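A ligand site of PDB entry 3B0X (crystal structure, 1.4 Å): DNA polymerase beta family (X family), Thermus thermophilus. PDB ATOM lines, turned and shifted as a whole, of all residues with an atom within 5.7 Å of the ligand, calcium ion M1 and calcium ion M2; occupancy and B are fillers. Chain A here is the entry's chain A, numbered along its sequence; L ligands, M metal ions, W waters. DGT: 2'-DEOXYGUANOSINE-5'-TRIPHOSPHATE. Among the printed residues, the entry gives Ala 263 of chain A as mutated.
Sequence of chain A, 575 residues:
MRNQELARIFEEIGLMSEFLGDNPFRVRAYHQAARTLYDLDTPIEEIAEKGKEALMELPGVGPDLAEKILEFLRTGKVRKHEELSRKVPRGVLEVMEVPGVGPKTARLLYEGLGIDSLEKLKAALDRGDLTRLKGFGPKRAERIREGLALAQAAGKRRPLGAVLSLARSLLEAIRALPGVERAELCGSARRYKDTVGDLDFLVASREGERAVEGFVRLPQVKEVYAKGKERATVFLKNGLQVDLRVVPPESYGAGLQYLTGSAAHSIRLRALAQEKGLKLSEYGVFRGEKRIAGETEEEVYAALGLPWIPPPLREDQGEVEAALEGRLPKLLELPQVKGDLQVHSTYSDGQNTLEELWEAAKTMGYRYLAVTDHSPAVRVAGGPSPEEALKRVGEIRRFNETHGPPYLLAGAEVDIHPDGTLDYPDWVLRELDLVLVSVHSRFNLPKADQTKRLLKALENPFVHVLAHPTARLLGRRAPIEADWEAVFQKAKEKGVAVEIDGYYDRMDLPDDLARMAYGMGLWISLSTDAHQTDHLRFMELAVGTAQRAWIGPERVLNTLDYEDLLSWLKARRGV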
ATOM      1  N   MET A   1      16.126 -29.253  24.327  1.00  0.00           N
ATOM      2  CA  MET A   1      17.536 -29.321  24.815  1.00  0.00           C
ATOM      3  C   MET A   1      17.650 -28.994  26.289  1.00  0.00           C
ATOM      4  O   MET A   1      16.901 -28.162  26.809  1.00  0.00           O
ATOM      5  CB  MET A   1      18.424 -28.371  24.015  1.00  0.00           C
ATOM      6  CG  MET A   1      18.972 -28.989  22.757  1.00  0.00           C
ATOM      7  SD  MET A   1      20.270 -27.967  22.055  1.00  0.00           S
ATOM      8  CE  MET A   1      19.316 -27.000  20.888  1.00  0.00           C
ATOM      9  N   ARG A 157       6.743  -8.433  34.879  1.00  0.00           N
ATOM     10  CA  ARG A 157       6.309  -8.159  33.497  1.00  0.00           C
ATOM     11  C   ARG A 157       5.925  -6.697  33.372  1.00  0.00           C
ATOM     12  O   ARG A 157       5.526  -6.086  34.356  1.00  0.00           O
ATOM     13  CB  ARG A 157       5.163  -9.089  33.110  1.00  0.00           C
ATOM     14  CG  ARG A 157       5.500 -10.564  33.369  1.00  0.00           C
ATOM     15  CD  ARG A 157       4.402 -11.503  32.915  1.00  0.00           C
ATOM     16  NE  ARG A 157       4.252 -11.507  31.462  1.00  0.00           N
ATOM     17  CZ  ARG A 157       5.010 -12.193  30.623  1.00  0.00           C
ATOM     18  NH1 ARG A 157       5.984 -12.979  31.062  1.00  0.00           N
ATOM     19  NH2 ARG A 157       4.769 -12.135  29.325  1.00  0.00           N
ATOM     20  N   CYS A 186      11.539 -10.330  18.519  1.00  0.00           N
ATOM     21  CA  CYS A 186      10.760 -11.556  18.549  1.00  0.00           C
ATOM     22  C   CYS A 186      10.100 -11.756  19.917  1.00  0.00           C
ATOM     23  O   CYS A 186       9.593 -10.796  20.508  1.00  0.00           O
ATOM     24  CB  CYS A 186      11.629 -12.738  18.087  1.00  0.00           C
ATOM     25  SG  CYS A 186      12.217 -12.570  16.372  1.00  0.00           S
ATOM     26  N   GLY A 187      10.090 -12.984  20.415  1.00  0.00           N
ATOM     27  CA  GLY A 187       9.465 -13.322  21.684  1.00  0.00           C
ATOM     28  C   GLY A 187       8.010 -12.904  21.749  1.00  0.00           C
ATOM     29  O   GLY A 187       7.321 -12.701  20.731  1.00  0.00           O
ATOM     30  N   SER A 188       7.521 -12.746  22.975  1.00  0.00           N
ATOM     31  CA  SER A 188       6.097 -12.439  23.202  1.00  0.00           C
ATOM     32  C   SER A 188       5.719 -11.044  22.676  1.00  0.00           C
ATOM     33  O   SER A 188       4.555 -10.820  22.324  1.00  0.00           O
ATOM     34  CB  SER A 188       5.760 -12.571  24.670  1.00  0.00           C
ATOM     35  OG  SER A 188       6.544 -11.658  25.417  1.00  0.00           O
ATOM     36  N   ALA A 189       6.699 -10.141  22.547  1.00  0.00           N
ATOM     37  CA  ALA A 189       6.420  -8.828  21.985  1.00  0.00           C
ATOM     38  C   ALA A 189       5.941  -8.947  20.539  1.00  0.00           C
ATOM     39  O   ALA A 189       4.999  -8.260  20.142  1.00  0.00           O
ATOM     40  CB  ALA A 189       7.633  -7.923  22.061  1.00  0.00           C
ATOM     41  N   ARG A 191       4.349 -11.310  19.305  1.00  0.00           N
ATOM     42  CA  ARG A 191       3.014 -11.899  19.361  1.00  0.00           C
ATOM     43  C   ARG A 191       1.967 -10.918  19.919  1.00  0.00           C
ATOM     44  O   ARG A 191       0.799 -11.287  20.045  1.00  0.00           O
ATOM     45  CB  ARG A 191       3.004 -13.198  20.157  1.00  0.00           C
ATOM     46  CG  ARG A 191       4.080 -14.201  19.694  1.00  0.00           C
ATOM     47  CD  ARG A 191       3.781 -15.623  20.142  1.00  0.00           C
ATOM     48  NE  ARG A 191       3.498 -15.732  21.571  1.00  0.00           N
ATOM     49  CZ  ARG A 191       4.406 -15.815  22.544  1.00  0.00           C
ATOM     50  NH1 ARG A 191       5.715 -15.834  22.297  1.00  0.00           N
ATOM     51  NH2 ARG A 191       3.993 -15.848  23.831  1.00  0.00           N
ATOM     52  N   LYS A 193       1.521  -9.886  22.911  1.00  0.00           N
ATOM     53  CA  LYS A 193       1.081 -10.183  24.276  1.00  0.00           C
ATOM     54  C   LYS A 193       1.067  -8.904  25.086  1.00  0.00           C
ATOM     55  O   LYS A 193       1.962  -8.069  24.924  1.00  0.00           O
ATOM     56  CB  LYS A 193       2.027 -11.189  24.882  1.00  0.00           C
ATOM     57  CG  LYS A 193       1.457 -11.877  26.114  1.00  0.00           C
ATOM     58  CD  LYS A 193       2.394 -12.980  26.584  1.00  0.00           C
ATOM     59  CE  LYS A 193       1.904 -13.624  27.867  1.00  0.00           C
ATOM     60  NZ  LYS A 193       0.761 -14.535  27.534  1.00  0.00           N
ATOM     61  N   THR A 195       1.526  -8.048  28.218  1.00  0.00           N
ATOM     62  CA  THR A 195       2.632  -7.805  29.134  1.00  0.00           C
ATOM     63  C   THR A 195       3.751  -8.712  28.671  1.00  0.00           C
ATOM     64  O   THR A 195       3.505  -9.793  28.115  1.00  0.00           O
ATOM     65  CB  THR A 195       2.308  -8.083  30.613  1.00  0.00           C
ATOM     66  OG1 THR A 195       2.150  -9.485  30.845  1.00  0.00           O
ATOM     67  CG2 THR A 195       1.062  -7.303  31.064  1.00  0.00           C
ATOM     68  N   VAL A 196       4.983  -8.278  28.900  1.00  0.00           N
ATOM     69  CA  VAL A 196       6.155  -9.004  28.426  1.00  0.00           C
ATOM     70  C   VAL A 196       7.168  -9.165  29.530  1.00  0.00           C
ATOM     71  O   VAL A 196       7.295  -8.294  30.405  1.00  0.00           O
ATOM     72  CB  VAL A 196       6.793  -8.334  27.189  1.00  0.00           C
ATOM     73  CG1 VAL A 196       5.813  -8.327  26.026  1.00  0.00           C
ATOM     74  CG2 VAL A 196       7.274  -6.916  27.526  1.00  0.00           C
ATOM     75  N   GLY A 197       7.916 -10.258  29.457  1.00  0.00           N
ATOM     76  CA  GLY A 197       9.112 -10.442  30.287  1.00  0.00           C
ATOM     77  C   GLY A 197      10.271  -9.790  29.582  1.00  0.00           C
ATOM     78  O   GLY A 197      10.200  -8.645  29.141  1.00  0.00           O
ATOM     79  N   ASP A 198      11.380 -10.513  29.465  1.00  0.00           N
ATOM     80  CA  ASP A 198      12.522  -9.964  28.739  1.00  0.00           C
ATOM     81  C   ASP A 198      12.217  -9.777  27.243  1.00  0.00           C
ATOM     82  O   ASP A 198      11.224 -10.307  26.725  1.00  0.00           O
ATOM     83  CB  ASP A 198      13.799 -10.778  28.968  1.00  0.00           C
ATOM     84  CG  ASP A 198      13.738 -12.173  28.360  1.00  0.00           C
ATOM     85  OD1 ASP A 198      12.865 -12.480  27.519  1.00  0.00           O
ATOM     86  OD2 ASP A 198      14.589 -13.003  28.724  1.00  0.00           O
ATOM     87  N   LEU A 199      13.038  -8.957  26.584  1.00  0.00           N
ATOM     88  CA  LEU A 199      12.894  -8.742  25.140  1.00  0.00           C
ATOM     89  C   LEU A 199      13.906  -9.579  24.407  1.00  0.00           C
ATOM     90  O   LEU A 199      15.027  -9.726  24.875  1.00  0.00           O
ATOM     91  CB  LEU A 199      13.102  -7.279  24.807  1.00  0.00           C
ATOM     92  CG  LEU A 199      11.970  -6.445  25.430  1.00  0.00           C
ATOM     93  CD1 LEU A 199      12.455  -5.030  25.534  1.00  0.00           C
ATOM     94  CD2 LEU A 199      10.666  -6.507  24.677  1.00  0.00           C
ATOM     95  N   ASP A 200      13.503 -10.157  23.270  1.00  0.00           N
ATOM     96  CA  ASP A 200      14.332 -11.117  22.554  1.00  0.00           C
ATOM     97  C   ASP A 200      14.515 -10.643  21.133  1.00  0.00           C
ATOM     98  O   ASP A 200      13.514 -10.379  20.450  1.00  0.00           O
ATOM     99  CB  ASP A 200      13.618 -12.474  22.534  1.00  0.00           C
ATOM    100  CG  ASP A 200      13.215 -12.897  23.904  1.00  0.00           C
ATOM    101  OD1 ASP A 200      14.049 -13.508  24.585  1.00  0.00           O
ATOM    102  OD2 ASP A 200      12.077 -12.605  24.312  1.00  0.00           O
ATOM    103  N   ASP A 243      17.679 -10.381  25.506  1.00  0.00           N
ATOM    104  CA  ASP A 243      18.365 -11.514  24.952  1.00  0.00           C
ATOM    105  C   ASP A 243      18.571 -11.291  23.454  1.00  0.00           C
ATOM    106  O   ASP A 243      17.662 -10.838  22.741  1.00  0.00           O
ATOM    107  CB  ASP A 243      17.515 -12.770  25.085  1.00  0.00           C
ATOM    108  CG  ASP A 243      17.453 -13.306  26.486  1.00  0.00           C
ATOM    109  OD1 ASP A 243      18.279 -12.974  27.353  1.00  0.00           O
ATOM    110  OD2 ASP A 243      16.536 -14.132  26.740  1.00  0.00           O
ATOM    111  N   TYR A 258      11.644 -19.826  15.728  1.00  0.00           N
ATOM    112  CA  TYR A 258      12.140 -20.276  17.015  1.00  0.00           C
ATOM    113  C   TYR A 258      11.959 -19.200  18.093  1.00  0.00           C
ATOM    114  O   TYR A 258      11.432 -19.459  19.185  1.00  0.00           O
ATOM    115  CB  TYR A 258      13.603 -20.694  16.883  1.00  0.00           C
ATOM    116  CG  TYR A 258      14.210 -21.096  18.188  1.00  0.00           C
ATOM    117  CD1 TYR A 258      14.210 -22.429  18.598  1.00  0.00           C
ATOM    118  CD2 TYR A 258      14.766 -20.143  19.037  1.00  0.00           C
ATOM    119  CE1 TYR A 258      14.752 -22.794  19.832  1.00  0.00           C
ATOM    120  CE2 TYR A 258      15.298 -20.485  20.269  1.00  0.00           C
ATOM    121  CZ  TYR A 258      15.294 -21.812  20.651  1.00  0.00           C
ATOM    122  OH  TYR A 258      15.828 -22.181  21.870  1.00  0.00           O
ATOM    123  N   LEU A 259      12.474 -18.010  17.818  1.00  0.00           N
ATOM    124  CA  LEU A 259      12.518 -16.992  18.857  1.00  0.00           C
ATOM    125  C   LEU A 259      11.184 -16.287  19.099  1.00  0.00           C
ATOM    126  O   LEU A 259      11.007 -15.578  20.107  1.00  0.00           O
ATOM    127  CB  LEU A 259      13.630 -15.985  18.560  1.00  0.00           C
ATOM    128  CG  LEU A 259      14.122 -15.174  19.757  1.00  0.00           C
ATOM    129  CD1 LEU A 259      14.531 -16.037  20.893  1.00  0.00           C
ATOM    130  CD2 LEU A 259      15.224 -14.224  19.331  1.00  0.00           C
ATOM    131  N   THR A 260      10.235 -16.480  18.189  1.00  0.00           N
ATOM    132  CA  THR A 260       8.893 -15.892  18.349  1.00  0.00           C
ATOM    133  C   THR A 260       7.978 -16.781  19.172  1.00  0.00           C
ATOM    134  O   THR A 260       7.108 -16.290  19.889  1.00  0.00           O
ATOM    135  CB  THR A 260       8.287 -15.575  16.968  1.00  0.00           C
ATOM    136  OG1 THR A 260       9.128 -14.601  16.324  1.00  0.00           O
ATOM    137  CG2 THR A 260       6.881 -15.016  17.056  1.00  0.00           C
ATOM    138  N   GLY A 261       8.180 -18.088  19.076  1.00  0.00           N
ATOM    139  CA  GLY A 261       7.344 -19.023  19.814  1.00  0.00           C
ATOM    140  C   GLY A 261       5.874 -18.826  19.463  1.00  0.00           C
ATOM    141  O   GLY A 261       5.535 -18.515  18.332  1.00  0.00           O
ATOM    142  N   SER A 262       4.948 -19.016  20.413  1.00  0.00           N
ATOM    143  CA  SER A 262       5.221 -19.491  21.757  1.00  0.00           C
ATOM    144  C   SER A 262       5.880 -20.872  21.751  1.00  0.00           C
ATOM    145  O   SER A 262       5.885 -21.589  20.726  1.00  0.00           O
ATOM    146  CB  SER A 262       3.913 -19.580  22.505  1.00  0.00           C
ATOM    147  OG  SER A 262       3.140 -20.677  22.031  1.00  0.00           O
ATOM    148  N   ALA A 263       6.411 -21.283  22.889  1.00  0.00           N
ATOM    149  CA  ALA A 263       6.990 -22.621  23.003  1.00  0.00           C
ATOM    150  C   ALA A 263       5.969 -23.687  22.622  1.00  0.00           C
ATOM    151  O   ALA A 263       6.329 -24.669  21.950  1.00  0.00           O
ATOM    152  CB  ALA A 263       7.542 -22.867  24.413  1.00  0.00           C
ATOM    153  N   SER A 266       5.720 -23.914  18.871  1.00  0.00           N
ATOM    154  CA  SER A 266       6.876 -24.589  18.300  1.00  0.00           C
ATOM    155  C   SER A 266       6.848 -26.103  18.522  1.00  0.00           C
ATOM    156  O   SER A 266       7.261 -26.872  17.648  1.00  0.00           O
ATOM    157  CB  SER A 266       8.178 -24.024  18.840  1.00  0.00           C
ATOM    158  OG  SER A 266       8.253 -22.671  18.498  1.00  0.00           O
ATOM    159  N   ARG A 270       7.324 -28.705  15.434  1.00  0.00           N
ATOM    160  CA  ARG A 270       8.380 -29.722  15.392  1.00  0.00           C
ATOM    161  C   ARG A 270       7.813 -31.130  15.147  1.00  0.00           C
ATOM    162  O   ARG A 270       8.438 -31.956  14.454  1.00  0.00           O
ATOM    163  CB  ARG A 270       9.240 -29.715  16.652  1.00  0.00           C
ATOM    164  CG  ARG A 270      10.173 -28.515  16.736  1.00  0.00           C
ATOM    165  CD  ARG A 270      11.281 -28.750  17.763  1.00  0.00           C
ATOM    166  NE  ARG A 270      10.714 -29.010  19.070  1.00  0.00           N
ATOM    167  CZ  ARG A 270      10.323 -28.075  19.933  1.00  0.00           C
ATOM    168  NH1 ARG A 270      10.459 -26.794  19.649  1.00  0.00           N
ATOM    169  NH2 ARG A 270       9.790 -28.454  21.087  1.00  0.00           N
HETATM  170  PG  DGT L   1       7.985 -13.695  28.024  1.00  0.00           P
HETATM  171  O1G DGT L   1       9.452 -13.350  27.923  1.00  0.00           O
HETATM  172  O2G DGT L   1       7.579 -14.460  29.264  1.00  0.00           O
HETATM  173  O3G DGT L   1       7.060 -12.498  27.812  1.00  0.00           O
HETATM  174  O3B DGT L   1       7.597 -14.672  26.787  1.00  0.00           O
HETATM  175  PB  DGT L   1       8.512 -15.120  25.557  1.00  0.00           P
HETATM  176  O1B DGT L   1       7.654 -15.924  24.638  1.00  0.00           O
HETATM  177  O2B DGT L   1       9.277 -13.969  24.989  1.00  0.00           O
HETATM  178  O3A DGT L   1       9.527 -16.156  26.258  1.00  0.00           O
HETATM  179  PA  DGT L   1      11.119 -16.267  26.431  1.00  0.00           P
HETATM  180  O1A DGT L   1      11.755 -14.920  26.436  1.00  0.00           O
HETATM  181  O2A DGT L   1      11.344 -17.175  27.617  1.00  0.00           O
HETATM  182  O5' DGT L   1      11.586 -17.106  25.172  1.00  0.00           O
HETATM  183  C5' DGT L   1      11.551 -16.483  23.867  1.00  0.00           C
HETATM  184  C4' DGT L   1      11.150 -17.495  22.813  1.00  0.00           C
HETATM  185  O4' DGT L   1      12.135 -18.518  22.771  1.00  0.00           O
HETATM  186  C3' DGT L   1       9.857 -18.233  23.051  1.00  0.00           C
HETATM  187  O3' DGT L   1       8.710 -17.511  22.627  1.00  0.00           O
HETATM  188  C2' DGT L   1      10.032 -19.493  22.247  1.00  0.00           C
HETATM  189  C1' DGT L   1      11.526 -19.755  22.386  1.00  0.00           C
HETATM  190  N9  DGT L   1      11.792 -20.737  23.441  1.00  0.00           N
HETATM  191  C8  DGT L   1      11.857 -20.486  24.775  1.00  0.00           C
HETATM  192  N7  DGT L   1      12.121 -21.637  25.438  1.00  0.00           N
HETATM  193  C5  DGT L   1      12.238 -22.608  24.514  1.00  0.00           C
HETATM  194  C6  DGT L   1      12.510 -24.055  24.539  1.00  0.00           C
HETATM  195  O6  DGT L   1      12.721 -24.647  25.618  1.00  0.00           O
HETATM  196  N1  DGT L   1      12.537 -24.681  23.363  1.00  0.00           N
HETATM  197  C2  DGT L   1      12.314 -24.055  22.183  1.00  0.00           C
HETATM  198  N2  DGT L   1      12.352 -24.777  21.058  1.00  0.00           N
HETATM  199  N3  DGT L   1      12.036 -22.738  22.058  1.00  0.00           N
HETATM  200  C4  DGT L   1      12.019 -21.997  23.199  1.00  0.00           C
HETATM  201 CA    CA M   1      10.858 -12.672  26.225  1.00  0.00          CA
HETATM  202 CA    CA M   2      14.186 -14.473  26.751  1.00  0.00          CA
HETATM  203  O   HOH W   1      12.824 -27.532  23.345  1.00  0.00           O
HETATM  204  O   HOH W   2      13.915 -15.920  28.551  1.00  0.00           O
HETATM  205  O   HOH W   3      13.128 -19.290  27.707  1.00  0.00           O
HETATM  206  O   HOH W   4       9.212 -11.038  25.180  1.00  0.00           O
HETATM  207  O   HOH W   5       5.559 -17.190  25.762  1.00  0.00           O
HETATM  208  O   HOH W   6      14.739 -16.510  25.687  1.00  0.00           O
HETATM  209  O   HOH W   7       9.405 -18.566  28.761  1.00  0.00           O
HETATM  210  O   HOH W   8      10.299 -21.787  19.948  1.00  0.00           O
HETATM  211  O   HOH W   9      12.269 -25.314  17.979  1.00  0.00           O
HETATM  212  O   HOH W  10      14.008 -27.247  20.921  1.00  0.00           O
HETATM  213  O   HOH W  11       9.099 -25.497  22.122  1.00  0.00           O
HETATM  214  O   HOH W  12      11.073 -13.363  30.150  1.00  0.00           O
HETATM  215  O   HOH W  13       5.229 -15.971  28.678  1.00  0.00           O
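Calcium ion M1 is bound by OD2 of Asp 200 (2.3 Å).
Calcium ion M1 is bound by O1G of the ligand (2.3 Å).
An oxygen (O2B) of the ligand binds calcium ion M1 (2.4 Å).
Calcium ion M1 is bound by OD1 of Asp 198 (2.4 Å).
An oxygen (O1A) of the ligand is bound to calcium ion M1 (2.4 Å).
O of Asp 198 binds calcium ion M1 (2.4 Å).
Water W4 is bound to calcium ion M1 (2.5 Å).
NH1 of Arg 270 lies close to N2 of the ligand.
CA of Gly 187 touches O2B of the ligand, at 3.4 Å.
Val 196 touches the ligand (CA to O3G, 3.7 Å).
Tyr 258 touches the ligand.
Leu 259 touches the ligand (O to C4', 3.3 Å).
Gly 261 touches the ligand (CA to O3', 3.5 Å).
Hydrophobic or aromatic side chains that line the ligand: Tyr 258 and Leu 259.
13 residues have an atom within 4 Å of the ligand: Arg 157, Gly 187, Ser 188, Arg 191, Val 196, Gly 197, Asp 198, Asp 200, Tyr 258, Leu 259, Thr 260, Gly 261 and Arg 270.
Calcium ion M2 is bound by water W2 (2.3 Å), water W6 (2.4 Å), OD2 of Asp 243 (2.4 Å), OD1 of Asp 200 (2.4 Å), O1A of the ligand (2.5 Å), OD2 of Asp 198 (2.5 Å) and OD1 of Asp 198 (2.5 Å).
Calcium ion M2 has seven donor atoms within binding distance.
The backbone NH of Cys 186 is in hydrogen-bond range of the backbone carbonyl oxygen of Asp 200.
O of Thr 195 sits at hydrogen-bond distance from NH2 of Arg 157, 2.9 Å away.
The guanidinium group of Arg 191 lies within hydrogen-bond range of the backbone carbonyl oxygen of Thr 260 (2.8 Å).
The backbone NH of Gly 187 sits at hydrogen-bond distance from the backbone carbonyl oxygen of Leu 259.
SG of Cys 186 lies close to OG1 of Thr 260, 3.7 Å away.
O of Ser 188 lies within hydrogen-bond range of N of Lys 193.
The backbone NH of Asp 243 lies within hydrogen-bond range of the backbone carbonyl oxygen of Leu 199 (2.8 Å).
Within 4 Å of calcium ion M2: Asp 198, Asp 200 and Asp 243.
The nearest printed residue that does not touch calcium ion M2 is Leu 199 (5.2 Å).
Two residues have an atom within 4 Å of calcium ion M1: Asp 198 and Asp 200.
The nearest printed residue that does not touch calcium ion M1 is Leu 199 (4.3 Å).
Water W5 bridges O1B of the ligand (2.7 Å) and NH2 of Arg 191 (2.8 Å).
Water W8 lies within hydrogen-bond range of OG of Ser 266 (2.7 Å), O of Tyr 258 (2.7 Å) and N3 of the ligand (2.9 Å).
Water W9 lies within hydrogen-bond range of the guanidinium group (NH1) of Arg 270 and a nitrogen (N2) of the ligand.
Water W11 lies within hydrogen-bond range of the backbone carbonyl oxygen of Ala 263 (2.9 Å), the guanidinium group of Arg 270 (3.1 Å) and a nitrogen (N2) of the ligand (3.5 Å).
OG of Ser 188 lies within hydrogen-bond range of O3G of the ligand, 2.6 Å away.
The guanidinium group (NH1) of Arg 191 is in salt-bridge range of an oxygen (O1B) of the ligand (3.0 Å).
The backbone NH of Ser 188 lies close to an oxygen (O2B) of the ligand, 2.9 Å away.
An oxygen (O3G) of the ligand sits at hydrogen-bond distance from the backbone NH (N) of Gly 197 (2.9 Å).
An oxygen (O3') of the ligand is in hydrogen-bond range of the backbone carbonyl oxygen of Thr 260 (3.4 Å).
NH2 of Arg 157 is in salt-bridge range of O3G of the ligand, at 2.8 Å.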
